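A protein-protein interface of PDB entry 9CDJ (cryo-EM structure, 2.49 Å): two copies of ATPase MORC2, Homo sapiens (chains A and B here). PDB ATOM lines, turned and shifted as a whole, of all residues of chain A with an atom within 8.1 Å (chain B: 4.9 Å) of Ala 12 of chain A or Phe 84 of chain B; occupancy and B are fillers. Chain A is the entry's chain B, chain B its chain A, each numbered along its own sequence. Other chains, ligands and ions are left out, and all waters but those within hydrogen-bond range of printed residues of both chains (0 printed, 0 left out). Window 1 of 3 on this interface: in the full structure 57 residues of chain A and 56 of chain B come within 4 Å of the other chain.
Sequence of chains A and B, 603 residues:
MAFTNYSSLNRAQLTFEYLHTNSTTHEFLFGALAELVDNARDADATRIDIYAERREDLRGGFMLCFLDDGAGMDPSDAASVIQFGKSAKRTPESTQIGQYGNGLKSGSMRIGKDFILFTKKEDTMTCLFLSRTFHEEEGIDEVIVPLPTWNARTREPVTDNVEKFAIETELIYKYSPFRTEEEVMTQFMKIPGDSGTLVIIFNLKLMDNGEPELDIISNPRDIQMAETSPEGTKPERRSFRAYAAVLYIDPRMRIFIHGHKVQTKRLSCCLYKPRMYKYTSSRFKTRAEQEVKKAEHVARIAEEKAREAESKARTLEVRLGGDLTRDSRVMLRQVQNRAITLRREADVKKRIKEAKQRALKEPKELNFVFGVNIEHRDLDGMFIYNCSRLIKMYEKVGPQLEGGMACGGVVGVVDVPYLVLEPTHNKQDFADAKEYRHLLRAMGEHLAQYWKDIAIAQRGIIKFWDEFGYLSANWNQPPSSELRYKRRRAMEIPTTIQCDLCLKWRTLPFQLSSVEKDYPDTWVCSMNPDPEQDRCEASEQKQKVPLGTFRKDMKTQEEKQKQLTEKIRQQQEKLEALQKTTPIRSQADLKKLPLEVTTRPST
The backbone NH (N) of Lys 86 of chain B lies within hydrogen-bond range of the side-chain hydroxyl (OG1) of Thr 15 of chain A, at 3.4 Å. The side-chain hydroxyl of Tyr 18 of chain B lies within hydrogen-bond range of the side-chain hydroxyl of Tyr 18 of chain A (2.8 Å). The side-chain hydroxyl (OH) of Tyr 18 of chain A lies close to the side-chain amide oxygen (OD1) of Asn 102 of chain B (3.2 Å). The backbone carbonyl oxygen (O) of Phe 84 of chain B sits at hydrogen-bond distance from the backbone NH (N) of Thr 15 of chain A. The backbone NH of Ala 12 of chain A sits at hydrogen-bond distance from the backbone carbonyl oxygen of Val 143 of chain B, at 2.7 Å. The side-chain hydroxyl of Thr 21 of chain A is in hydrogen-bond range of the backbone carbonyl oxygen of Tyr 100 of chain B (2.9 Å). OD1 of Asn 22 of chain B lies within hydrogen-bond range of OH of Tyr 18 of chain A (3.2 Å). N of Val 145 of chain B sits at hydrogen-bond distance from O of Asn 10 of chain A (3.0 Å). The backbone NH (N) of Gln 13 of chain A is in hydrogen-bond range of the backbone carbonyl oxygen (O) of Ile 82 of chain B. The backbone carbonyl oxygen (O) of Gln 13 of chain A lies within hydrogen-bond range of the backbone NH (N) of Phe 84 of chain B (2.9 Å).
The backbone NH (N) of Gly 85 of chain B is in hydrogen-bond range of the backbone carbonyl oxygen (O) of Gly 101 of chain B (3.1 Å). The side-chain amide oxygen (OD1) of Asn 102 of chain B sits at hydrogen-bond distance from the side-chain amide nitrogen (ND2) of Asn 22 of chain B. The guanidinium group (NH1) of Arg 11 of chain A is in hydrogen-bond range of the backbone carbonyl oxygen (O) of Leu 9 of chain A, at 2.9 Å. N of Gly 85 of chain B lies close to O of Tyr 100 of chain B (3.5 Å).
Asn 10 of chain A touches Ile 82 of chain B (CB to CD1, 3.8 Å). O of Arg 11 of chain A touches CD1 of Ile 82 of chain B, at 3.8 Å. Arg 11 of chain A touches Val 143 of chain B (CA to O, 3.3 Å). O of Ala 12 of chain A touches CD1 of Leu 14 of chain B, 3.4 Å away. CG of Gln 13 of chain A touches OE1 of Gln 83 of chain B (3.3 Å). Leu 14 of chain A touches Phe 84 of chain B. Thr 15 of chain A touches Gly 85 of chain B (OG1 to CA, 3.1 Å). Phe 84 of chain B touches Tyr 18 of chain A. Leu 14 of chain B touches Phe 84 of chain A (C to O, 3.8 Å). Phe 84 of chain A touches Tyr 18 of chain B.
Of the printed residues of chain B, Arg 11 of chain A touches Ile 82 and Val 143. Of chain B, only Leu 14 (3.4 Å), Ile 82 (3.3 Å), Phe 84 (3.8 Å) and Val 143 (2.7 Å) come within 4 Å of Ala 12 of chain A. Printed residues of chain B within 4 Å of Leu 14 of chain A: Leu 14 and Phe 84. Phe 16 of chain A touches none of the printed residues of chain B. Of the printed residues of chain B, Glu 17 of chain A touches Gly 85 (3.5 Å). Printed residues of chain A within 4 Å of Leu 14 of chain B: Ala 12, Leu 14 and Phe 84. Printed residues of chain A within 4 Å of Tyr 18 of chain B: Tyr 18 and Phe 84. Leu 19 of chain B touches none of the printed residues of chain A. Phe 84 of chain B touches just these residues of chain A: Ala 12 (3.8 Å), Gln 13 (2.9 Å), Leu 14 (3.9 Å), Thr 15 (2.3 Å) and Tyr 18 (3.3 Å). The nearest printed residue of chain A that does not touch Lys 86 of chain B is Asp 141 of chain A (4.2 Å).
Hydrophobic or aromatic side chains of chain A within 4 Å of the printed part of chain B: Ala 12, Leu 14, Tyr 18 and Phe 84. Of the 16 printed residues of chain B, 12 touch a printed residue of chain A. Printed residues of chain B that touch a printed residue of chain A: Leu 14, Tyr 18, Asn 22, Ile 82, Gln 83, Phe 84, Gly 85, Lys 86, Tyr 100, Asn 102, Val 143 and Val 145. Hydrophobic or aromatic side chains of chain B that line the printed part of chain A: Leu 14, Tyr 18, Ile 82, Phe 84, Tyr 100 and Val 143.
Leu 14 of chain B touches its own counterpart, Leu 14 of chain A. Leu 14 of chain A touches Phe 84 of chain B, and with the chains exchanged Phe 84 of chain A touches Leu 14 of chain B. Tyr 18 of chain B touches its own counterpart, Tyr 18 of chain A. Tyr 18 of chain A touches Phe 84 of chain B, and with the chains exchanged Phe 84 of chain A touches Tyr 18 of chain B. Positions printed for both chains: 14, 18, 19, 84 and 143.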
ATOM      1  N   LEU A   9      -7.040 -31.768  -7.821  1.00  0.00           N
ATOM      2  CA  LEU A   9      -7.996 -30.820  -8.370  1.00  0.00           C
ATOM      3  C   LEU A   9      -7.303 -29.535  -8.801  1.00  0.00           C
ATOM      4  O   LEU A   9      -6.256 -29.157  -8.269  1.00  0.00           O
ATOM      5  CB  LEU A   9      -9.086 -30.491  -7.349  1.00  0.00           C
ATOM      6  CG  LEU A   9      -9.935 -31.656  -6.838  1.00  0.00           C
ATOM      7  CD1 LEU A   9     -11.188 -31.128  -6.160  1.00  0.00           C
ATOM      8  CD2 LEU A   9     -10.289 -32.611  -7.961  1.00  0.00           C
ATOM      9  N   ASN A  10      -7.902 -28.864  -9.781  1.00  0.00           N
ATOM     10  CA  ASN A  10      -7.375 -27.589 -10.243  1.00  0.00           C
ATOM     11  C   ASN A  10      -7.494 -26.540  -9.147  1.00  0.00           C
ATOM     12  O   ASN A  10      -8.429 -26.558  -8.343  1.00  0.00           O
ATOM     13  CB  ASN A  10      -8.124 -27.126 -11.492  1.00  0.00           C
ATOM     14  CG  ASN A  10      -8.061 -28.135 -12.617  1.00  0.00           C
ATOM     15  OD1 ASN A  10      -8.629 -29.222 -12.522  1.00  0.00           O
ATOM     16  ND2 ASN A  10      -7.371 -27.779 -13.694  1.00  0.00           N
ATOM     17  N   ARG A  11      -6.534 -25.622  -9.117  1.00  0.00           N
ATOM     18  CA  ARG A  11      -6.522 -24.516  -8.173  1.00  0.00           C
ATOM     19  C   ARG A  11      -6.662 -23.206  -8.933  1.00  0.00           C
ATOM     20  O   ARG A  11      -6.103 -23.049 -10.021  1.00  0.00           O
ATOM     21  CB  ARG A  11      -5.226 -24.500  -7.359  1.00  0.00           C
ATOM     22  CG  ARG A  11      -5.328 -25.151  -5.994  1.00  0.00           C
ATOM     23  CD  ARG A  11      -4.992 -26.628  -6.068  1.00  0.00           C
ATOM     24  NE  ARG A  11      -4.982 -27.255  -4.753  1.00  0.00           N
ATOM     25  CZ  ARG A  11      -5.187 -28.547  -4.535  1.00  0.00           C
ATOM     26  NH1 ARG A  11      -5.411 -29.390  -5.530  1.00  0.00           N
ATOM     27  NH2 ARG A  11      -5.161 -29.006  -3.288  1.00  0.00           N
ATOM     28  N   ALA A  12      -7.419 -22.271  -8.366  1.00  0.00           N
ATOM     29  CA  ALA A  12      -7.483 -20.934  -8.937  1.00  0.00           C
ATOM     30  C   ALA A  12      -6.130 -20.262  -8.758  1.00  0.00           C
ATOM     31  O   ALA A  12      -5.721 -19.963  -7.631  1.00  0.00           O
ATOM     32  CB  ALA A  12      -8.586 -20.115  -8.274  1.00  0.00           C
ATOM     33  N   GLN A  13      -5.434 -20.026  -9.866  1.00  0.00           N
ATOM     34  CA  GLN A  13      -4.058 -19.560  -9.843  1.00  0.00           C
ATOM     35  C   GLN A  13      -3.980 -18.115 -10.305  1.00  0.00           C
ATOM     36  O   GLN A  13      -4.744 -17.676 -11.170  1.00  0.00           O
ATOM     37  CB  GLN A  13      -3.167 -20.426 -10.737  1.00  0.00           C
ATOM     38  CG  GLN A  13      -3.381 -21.916 -10.571  1.00  0.00           C
ATOM     39  CD  GLN A  13      -2.088 -22.666 -10.347  1.00  0.00           C
ATOM     40  OE1 GLN A  13      -1.261 -22.783 -11.250  1.00  0.00           O
ATOM     41  NE2 GLN A  13      -1.904 -23.177  -9.136  1.00  0.00           N
ATOM     42  N   LEU A  14      -3.049 -17.379  -9.714  1.00  0.00           N
ATOM     43  CA  LEU A  14      -2.759 -16.023 -10.143  1.00  0.00           C
ATOM     44  C   LEU A  14      -1.907 -16.043 -11.403  1.00  0.00           C
ATOM     45  O   LEU A  14      -1.190 -17.005 -11.687  1.00  0.00           O
ATOM     46  CB  LEU A  14      -2.030 -15.249  -9.045  1.00  0.00           C
ATOM     47  CG  LEU A  14      -2.876 -14.621  -7.938  1.00  0.00           C
ATOM     48  CD1 LEU A  14      -2.018 -13.688  -7.112  1.00  0.00           C
ATOM     49  CD2 LEU A  14      -4.082 -13.890  -8.498  1.00  0.00           C
ATOM     50  N   THR A  15      -1.995 -14.958 -12.164  1.00  0.00           N
ATOM     51  CA  THR A  15      -1.190 -14.774 -13.358  1.00  0.00           C
ATOM     52  C   THR A  15      -0.545 -13.398 -13.309  1.00  0.00           C
ATOM     53  O   THR A  15      -1.031 -12.493 -12.627  1.00  0.00           O
ATOM     54  CB  THR A  15      -2.028 -14.921 -14.635  1.00  0.00           C
ATOM     55  OG1 THR A  15      -3.092 -13.963 -14.626  1.00  0.00           O
ATOM     56  CG2 THR A  15      -2.611 -16.321 -14.728  1.00  0.00           C
ATOM     57  N   PHE A  16       0.563 -13.251 -14.037  1.00  0.00           N
ATOM     58  CA  PHE A  16       1.300 -11.994 -14.005  1.00  0.00           C
ATOM     59  C   PHE A  16       0.412 -10.811 -14.361  1.00  0.00           C
ATOM     60  O   PHE A  16       0.609  -9.708 -13.842  1.00  0.00           O
ATOM     61  CB  PHE A  16       2.488 -12.059 -14.963  1.00  0.00           C
ATOM     62  CG  PHE A  16       2.933 -10.718 -15.454  1.00  0.00           C
ATOM     63  CD1 PHE A  16       3.618  -9.855 -14.619  1.00  0.00           C
ATOM     64  CD2 PHE A  16       2.657 -10.312 -16.747  1.00  0.00           C
ATOM     65  CE1 PHE A  16       4.024  -8.619 -15.065  1.00  0.00           C
ATOM     66  CE2 PHE A  16       3.061  -9.075 -17.198  1.00  0.00           C
ATOM     67  CZ  PHE A  16       3.745  -8.227 -16.355  1.00  0.00           C
ATOM     68  N   GLU A  17      -0.571 -11.019 -15.236  1.00  0.00           N
ATOM     69  CA  GLU A  17      -1.470  -9.941 -15.627  1.00  0.00           C
ATOM     70  C   GLU A  17      -2.476  -9.609 -14.536  1.00  0.00           C
ATOM     71  O   GLU A  17      -3.004  -8.487 -14.507  1.00  0.00           O
ATOM     72  CB  GLU A  17      -2.214 -10.301 -16.918  1.00  0.00           C
ATOM     73  CG  GLU A  17      -1.414 -11.119 -17.939  1.00  0.00           C
ATOM     74  CD  GLU A  17      -0.547 -10.254 -18.834  1.00  0.00           C
ATOM     75  OE1 GLU A  17      -0.667  -9.013 -18.767  1.00  0.00           O
ATOM     76  OE2 GLU A  17       0.258 -10.819 -19.604  1.00  0.00           O
ATOM     77  N   TYR A  18      -2.750 -10.548 -13.632  1.00  0.00           N
ATOM     78  CA  TYR A  18      -3.658 -10.227 -12.546  1.00  0.00           C
ATOM     79  C   TYR A  18      -3.068  -9.196 -11.602  1.00  0.00           C
ATOM     80  O   TYR A  18      -3.819  -8.556 -10.869  1.00  0.00           O
ATOM     81  CB  TYR A  18      -4.048 -11.465 -11.749  1.00  0.00           C
ATOM     82  CG  TYR A  18      -5.199 -11.170 -10.819  1.00  0.00           C
ATOM     83  CD1 TYR A  18      -6.484 -11.010 -11.314  1.00  0.00           C
ATOM     84  CD2 TYR A  18      -4.997 -11.007  -9.459  1.00  0.00           C
ATOM     85  CE1 TYR A  18      -7.539 -10.725 -10.478  1.00  0.00           C
ATOM     86  CE2 TYR A  18      -6.047 -10.723  -8.615  1.00  0.00           C
ATOM     87  CZ  TYR A  18      -7.317 -10.581  -9.130  1.00  0.00           C
ATOM     88  OH  TYR A  18      -8.372 -10.294  -8.296  1.00  0.00           O
ATOM     89  N   LEU A  19      -1.748  -9.011 -11.599  1.00  0.00           N
ATOM     90  CA  LEU A  19      -1.177  -7.923 -10.812  1.00  0.00           C
ATOM     91  C   LEU A  19      -1.679  -6.577 -11.317  1.00  0.00           C
ATOM     92  O   LEU A  19      -2.140  -5.738 -10.533  1.00  0.00           O
ATOM     93  CB  LEU A  19       0.348  -7.988 -10.852  1.00  0.00           C
ATOM     94  CG  LEU A  19       0.967  -9.237 -10.220  1.00  0.00           C
ATOM     95  CD1 LEU A  19       2.454  -9.303 -10.513  1.00  0.00           C
ATOM     96  CD2 LEU A  19       0.713  -9.263  -8.722  1.00  0.00           C
ATOM     97  N   THR A  21      -4.383  -6.193 -13.164  1.00  0.00           N
ATOM     98  CA  THR A  21      -5.822  -6.210 -12.915  1.00  0.00           C
ATOM     99  C   THR A  21      -6.133  -5.724 -11.505  1.00  0.00           C
ATOM    100  O   THR A  21      -6.980  -4.846 -11.303  1.00  0.00           O
ATOM    101  CB  THR A  21      -6.375  -7.618 -13.126  1.00  0.00           C
ATOM    102  OG1 THR A  21      -6.480  -7.891 -14.529  1.00  0.00           O
ATOM    103  CG2 THR A  21      -7.740  -7.766 -12.471  1.00  0.00           C
ATOM    104  N   PHE A  84      -2.521 -13.859  -1.711  1.00  0.00           N
ATOM    105  CA  PHE A  84      -3.595 -12.901  -1.926  1.00  0.00           C
ATOM    106  C   PHE A  84      -4.835 -13.315  -1.145  1.00  0.00           C
ATOM    107  O   PHE A  84      -5.224 -14.484  -1.138  1.00  0.00           O
ATOM    108  CB  PHE A  84      -3.922 -12.799  -3.415  1.00  0.00           C
ATOM    109  CG  PHE A  84      -2.924 -12.004  -4.204  1.00  0.00           C
ATOM    110  CD1 PHE A  84      -1.580 -12.330  -4.182  1.00  0.00           C
ATOM    111  CD2 PHE A  84      -3.335 -10.939  -4.986  1.00  0.00           C
ATOM    112  CE1 PHE A  84      -0.666 -11.603  -4.915  1.00  0.00           C
ATOM    113  CE2 PHE A  84      -2.425 -10.211  -5.721  1.00  0.00           C
ATOM    114  CZ  PHE A  84      -1.090 -10.545  -5.687  1.00  0.00           C
ATOM    115  N   ASP A 141       4.293 -16.352 -16.824  1.00  0.00           N
ATOM    116  CA  ASP A 141       2.851 -16.205 -16.665  1.00  0.00           C
ATOM    117  C   ASP A 141       2.413 -16.278 -15.213  1.00  0.00           C
ATOM    118  O   ASP A 141       1.475 -15.576 -14.823  1.00  0.00           O
ATOM    119  CB  ASP A 141       2.103 -17.280 -17.464  1.00  0.00           C
ATOM    120  CG  ASP A 141       2.732 -18.654 -17.334  1.00  0.00           C
ATOM    121  OD1 ASP A 141       3.977 -18.746 -17.379  1.00  0.00           O
ATOM    122  OD2 ASP A 141       1.982 -19.641 -17.187  1.00  0.00           O
ATOM    123  N   VAL A 143       3.136 -15.704 -11.045  1.00  0.00           N
ATOM    124  CA  VAL A 143       3.656 -14.577 -10.280  1.00  0.00           C
ATOM    125  C   VAL A 143       4.688 -15.150  -9.318  1.00  0.00           C
ATOM    126  O   VAL A 143       4.352 -15.560  -8.200  1.00  0.00           O
ATOM    127  CB  VAL A 143       2.554 -13.815  -9.539  1.00  0.00           C
ATOM    128  CG1 VAL A 143       3.159 -12.764  -8.620  1.00  0.00           C
ATOM    129  CG2 VAL A 143       1.604 -13.167 -10.527  1.00  0.00           C
ATOM    130  N   LEU B  14      -3.507 -17.573  -4.721  1.00  0.00           N
ATOM    131  CA  LEU B  14      -4.809 -17.119  -4.274  1.00  0.00           C
ATOM    132  C   LEU B  14      -5.200 -17.830  -2.985  1.00  0.00           C
ATOM    133  O   LEU B  14      -4.675 -18.891  -2.638  1.00  0.00           O
ATOM    134  CB  LEU B  14      -5.861 -17.372  -5.350  1.00  0.00           C
ATOM    135  CG  LEU B  14      -5.835 -16.424  -6.545  1.00  0.00           C
ATOM    136  CD1 LEU B  14      -6.953 -16.762  -7.497  1.00  0.00           C
ATOM    137  CD2 LEU B  14      -5.937 -14.980  -6.097  1.00  0.00           C
ATOM    138  N   TYR B  18      -9.573 -14.403  -0.796  1.00  0.00           N
ATOM    139  CA  TYR B  18      -9.380 -13.477  -1.899  1.00  0.00           C
ATOM    140  C   TYR B  18     -10.565 -13.471  -2.847  1.00  0.00           C
ATOM    141  O   TYR B  18     -10.735 -12.502  -3.585  1.00  0.00           O
ATOM    142  CB  TYR B  18      -8.118 -13.790  -2.693  1.00  0.00           C
ATOM    143  CG  TYR B  18      -7.768 -12.648  -3.616  1.00  0.00           C
ATOM    144  CD1 TYR B  18      -7.287 -11.452  -3.107  1.00  0.00           C
ATOM    145  CD2 TYR B  18      -7.961 -12.746  -4.984  1.00  0.00           C
ATOM    146  CE1 TYR B  18      -6.980 -10.396  -3.935  1.00  0.00           C
ATOM    147  CE2 TYR B  18      -7.656 -11.694  -5.822  1.00  0.00           C
ATOM    148  CZ  TYR B  18      -7.166 -10.520  -5.290  1.00  0.00           C
ATOM    149  OH  TYR B  18      -6.861  -9.462  -6.112  1.00  0.00           O
ATOM    150  N   LEU B  19     -11.390 -14.517  -2.852  1.00  0.00           N
ATOM    151  CA  LEU B  19     -12.610 -14.464  -3.649  1.00  0.00           C
ATOM    152  C   LEU B  19     -13.518 -13.344  -3.159  1.00  0.00           C
ATOM    153  O   LEU B  19     -14.002 -12.529  -3.953  1.00  0.00           O
ATOM    154  CB  LEU B  19     -13.327 -15.812  -3.602  1.00  0.00           C
ATOM    155  CG  LEU B  19     -12.549 -16.979  -4.210  1.00  0.00           C
ATOM    156  CD1 LEU B  19     -13.243 -18.296  -3.912  1.00  0.00           C
ATOM    157  CD2 LEU B  19     -12.376 -16.791  -5.707  1.00  0.00           C
ATOM    158  N   ASN B  22     -11.823  -9.935  -3.983  1.00  0.00           N
ATOM    159  CA  ASN B  22     -12.106  -9.606  -5.373  1.00  0.00           C
ATOM    160  C   ASN B  22     -13.548  -9.157  -5.553  1.00  0.00           C
ATOM    161  O   ASN B  22     -13.819  -8.229  -6.324  1.00  0.00           O
ATOM    162  CB  ASN B  22     -11.808 -10.832  -6.240  1.00  0.00           C
ATOM    163  CG  ASN B  22     -11.750 -10.515  -7.715  1.00  0.00           C
ATOM    164  OD1 ASN B  22     -11.420  -9.402  -8.112  1.00  0.00           O
ATOM    165  ND2 ASN B  22     -12.065 -11.505  -8.540  1.00  0.00           N
ATOM    166  N   VAL B  81     -10.491 -20.051 -16.947  1.00  0.00           N
ATOM    167  CA  VAL B  81     -11.396 -19.179 -16.201  1.00  0.00           C
ATOM    168  C   VAL B  81     -10.825 -18.881 -14.823  1.00  0.00           C
ATOM    169  O   VAL B  81     -10.815 -17.729 -14.374  1.00  0.00           O
ATOM    170  CB  VAL B  81     -12.794 -19.813 -16.094  1.00  0.00           C
ATOM    171  CG1 VAL B  81     -13.685 -18.978 -15.189  1.00  0.00           C
ATOM    172  CG2 VAL B  81     -13.427 -19.956 -17.458  1.00  0.00           C
ATOM    173  N   ILE B  82     -10.340 -19.912 -14.127  1.00  0.00           N
ATOM    174  CA  ILE B  82      -9.828 -19.751 -12.773  1.00  0.00           C
ATOM    175  C   ILE B  82      -8.383 -19.289 -12.752  1.00  0.00           C
ATOM    176  O   ILE B  82      -7.804 -19.145 -11.667  1.00  0.00           O
ATOM    177  CB  ILE B  82      -9.985 -21.052 -11.960  1.00  0.00           C
ATOM    178  CG1 ILE B  82      -9.314 -22.230 -12.669  1.00  0.00           C
ATOM    179  CG2 ILE B  82     -11.455 -21.353 -11.739  1.00  0.00           C
ATOM    180  CD1 ILE B  82      -9.367 -23.515 -11.879  1.00  0.00           C
ATOM    181  N   GLN B  83      -7.777 -19.056 -13.916  1.00  0.00           N
ATOM    182  CA  GLN B  83      -6.484 -18.382 -13.997  1.00  0.00           C
ATOM    183  C   GLN B  83      -6.746 -16.881 -13.943  1.00  0.00           C
ATOM    184  O   GLN B  83      -6.917 -16.203 -14.959  1.00  0.00           O
ATOM    185  CB  GLN B  83      -5.737 -18.778 -15.264  1.00  0.00           C
ATOM    186  CG  GLN B  83      -5.500 -20.269 -15.413  1.00  0.00           C
ATOM    187  CD  GLN B  83      -4.496 -20.799 -14.412  1.00  0.00           C
ATOM    188  OE1 GLN B  83      -4.816 -21.651 -13.585  1.00  0.00           O
ATOM    189  NE2 GLN B  83      -3.269 -20.296 -14.483  1.00  0.00           N
ATOM    190  N   PHE B  84      -6.790 -16.358 -12.721  1.00  0.00           N
ATOM    191  CA  PHE B  84      -7.058 -14.941 -12.521  1.00  0.00           C
ATOM    192  C   PHE B  84      -6.054 -14.105 -13.298  1.00  0.00           C
ATOM    193  O   PHE B  84      -4.846 -14.342 -13.234  1.00  0.00           O
ATOM    194  CB  PHE B  84      -6.990 -14.601 -11.032  1.00  0.00           C
ATOM    195  CG  PHE B  84      -8.192 -15.044 -10.247  1.00  0.00           C
ATOM    196  CD1 PHE B  84      -8.610 -16.362 -10.271  1.00  0.00           C
ATOM    197  CD2 PHE B  84      -8.886 -14.142  -9.462  1.00  0.00           C
ATOM    198  CE1 PHE B  84      -9.706 -16.766  -9.539  1.00  0.00           C
ATOM    199  CE2 PHE B  84      -9.982 -14.542  -8.728  1.00  0.00           C
ATOM    200  CZ  PHE B  84     -10.390 -15.856  -8.765  1.00  0.00           C
ATOM    201  N   GLY B  85      -6.563 -13.126 -14.041  1.00  0.00           N
ATOM    202  CA  GLY B  85      -5.751 -12.302 -14.901  1.00  0.00           C
ATOM    203  C   GLY B  85      -5.583 -12.846 -16.303  1.00  0.00           C
ATOM    204  O   GLY B  85      -5.182 -12.095 -17.200  1.00  0.00           O
ATOM    205  N   LYS B  86      -5.880 -14.124 -16.516  1.00  0.00           N
ATOM    206  CA  LYS B  86      -5.779 -14.727 -17.837  1.00  0.00           C
ATOM    207  C   LYS B  86      -6.993 -14.326 -18.663  1.00  0.00           C
ATOM    208  O   LYS B  86      -8.133 -14.603 -18.276  1.00  0.00           O
ATOM    209  CB  LYS B  86      -5.681 -16.248 -17.723  1.00  0.00           C
ATOM    210  CG  LYS B  86      -5.440 -16.972 -19.042  1.00  0.00           C
ATOM    211  CD  LYS B  86      -4.092 -16.630 -19.660  1.00  0.00           C
ATOM    212  CE  LYS B  86      -2.935 -17.167 -18.831  1.00  0.00           C
ATOM    213  NZ  LYS B  86      -1.618 -16.873 -19.459  1.00  0.00           N
ATOM    214  N   TYR B 100      -9.274  -8.349 -17.974  1.00  0.00           N
ATOM    215  CA  TYR B 100      -8.637  -8.506 -16.680  1.00  0.00           C
ATOM    216  C   TYR B 100      -8.666  -9.932 -16.152  1.00  0.00           C
ATOM    217  O   TYR B 100      -8.105 -10.183 -15.081  1.00  0.00           O
ATOM    218  CB  TYR B 100      -9.317  -7.581 -15.661  1.00  0.00           C
ATOM    219  CG  TYR B 100      -9.153  -6.102 -15.951  1.00  0.00           C
ATOM    220  CD1 TYR B 100      -8.037  -5.619 -16.622  1.00  0.00           C
ATOM    221  CD2 TYR B 100     -10.122  -5.191 -15.559  1.00  0.00           C
ATOM    222  CE1 TYR B 100      -7.892  -4.272 -16.886  1.00  0.00           C
ATOM    223  CE2 TYR B 100      -9.984  -3.844 -15.821  1.00  0.00           C
ATOM    224  CZ  TYR B 100      -8.868  -3.389 -16.484  1.00  0.00           C
ATOM    225  OH  TYR B 100      -8.729  -2.047 -16.746  1.00  0.00           O
ATOM    226  N   GLY B 101      -9.305 -10.863 -16.857  1.00  0.00           N
ATOM    227  CA  GLY B 101      -9.393 -12.231 -16.391  1.00  0.00           C
ATOM    228  C   GLY B 101      -9.978 -12.321 -14.998  1.00  0.00           C
ATOM    229  O   GLY B 101      -9.668 -13.249 -14.245  1.00  0.00           O
ATOM    230  N   ASN B 102     -10.830 -11.361 -14.645  1.00  0.00           N
ATOM    231  CA  ASN B 102     -11.317 -11.238 -13.278  1.00  0.00           C
ATOM    232  C   ASN B 102     -12.826 -11.050 -13.211  1.00  0.00           C
ATOM    233  O   ASN B 102     -13.450 -11.394 -12.201  1.00  0.00           O
ATOM    234  CB  ASN B 102     -10.621 -10.065 -12.588  1.00  0.00           C
ATOM    235  CG  ASN B 102     -10.882 -10.029 -11.101  1.00  0.00           C
ATOM    236  OD1 ASN B 102     -10.622 -10.997 -10.390  1.00  0.00           O
ATOM    237  ND2 ASN B 102     -11.406  -8.909 -10.622  1.00  0.00           N
ATOM    238  N   LYS B 105     -15.274 -13.849 -11.948  1.00  0.00           N
ATOM    239  CA  LYS B 105     -15.091 -14.233 -10.555  1.00  0.00           C
ATOM    240  C   LYS B 105     -15.556 -13.125  -9.621  1.00  0.00           C
ATOM    241  O   LYS B 105     -16.295 -13.378  -8.661  1.00  0.00           O
ATOM    242  CB  LYS B 105     -13.625 -14.582 -10.302  1.00  0.00           C
ATOM    243  CG  LYS B 105     -13.205 -15.938 -10.860  1.00  0.00           C
ATOM    244  CD  LYS B 105     -12.936 -15.901 -12.360  1.00  0.00           C
ATOM    245  CE  LYS B 105     -11.716 -15.061 -12.698  1.00  0.00           C
ATOM    246  NZ  LYS B 105     -11.250 -15.288 -14.090  1.00  0.00           N
ATOM    247  N   VAL B 143      -8.132 -22.110  -3.363  1.00  0.00           N
ATOM    248  CA  VAL B 143      -9.353 -22.019  -4.153  1.00  0.00           C
ATOM    249  C   VAL B 143      -9.348 -23.218  -5.091  1.00  0.00           C
ATOM    250  O   VAL B 143      -8.784 -23.158  -6.190  1.00  0.00           O
ATOM    251  CB  VAL B 143      -9.451 -20.702  -4.927  1.00  0.00           C
ATOM    252  CG1 VAL B 143     -10.767 -20.630  -5.685  1.00  0.00           C
ATOM    253  CG2 VAL B 143      -9.315 -19.520  -3.983  1.00  0.00           C
ATOM    254  N   VAL B 145     -11.185 -25.689  -7.562  1.00  0.00           N
ATOM    255  CA  VAL B 145     -12.313 -25.543  -8.477  1.00  0.00           C
ATOM    256  C   VAL B 145     -12.454 -26.801  -9.324  1.00  0.00           C
ATOM    257  O   VAL B 145     -11.685 -26.992 -10.277  1.00  0.00           O
ATOM    258  CB  VAL B 145     -12.140 -24.298  -9.359  1.00  0.00           C
ATOM    259  CG1 VAL B 145     -13.378 -24.063 -10.206  1.00  0.00           C
ATOM    260  CG2 VAL B 145     -11.839 -23.086  -8.492  1.00  0.00           C
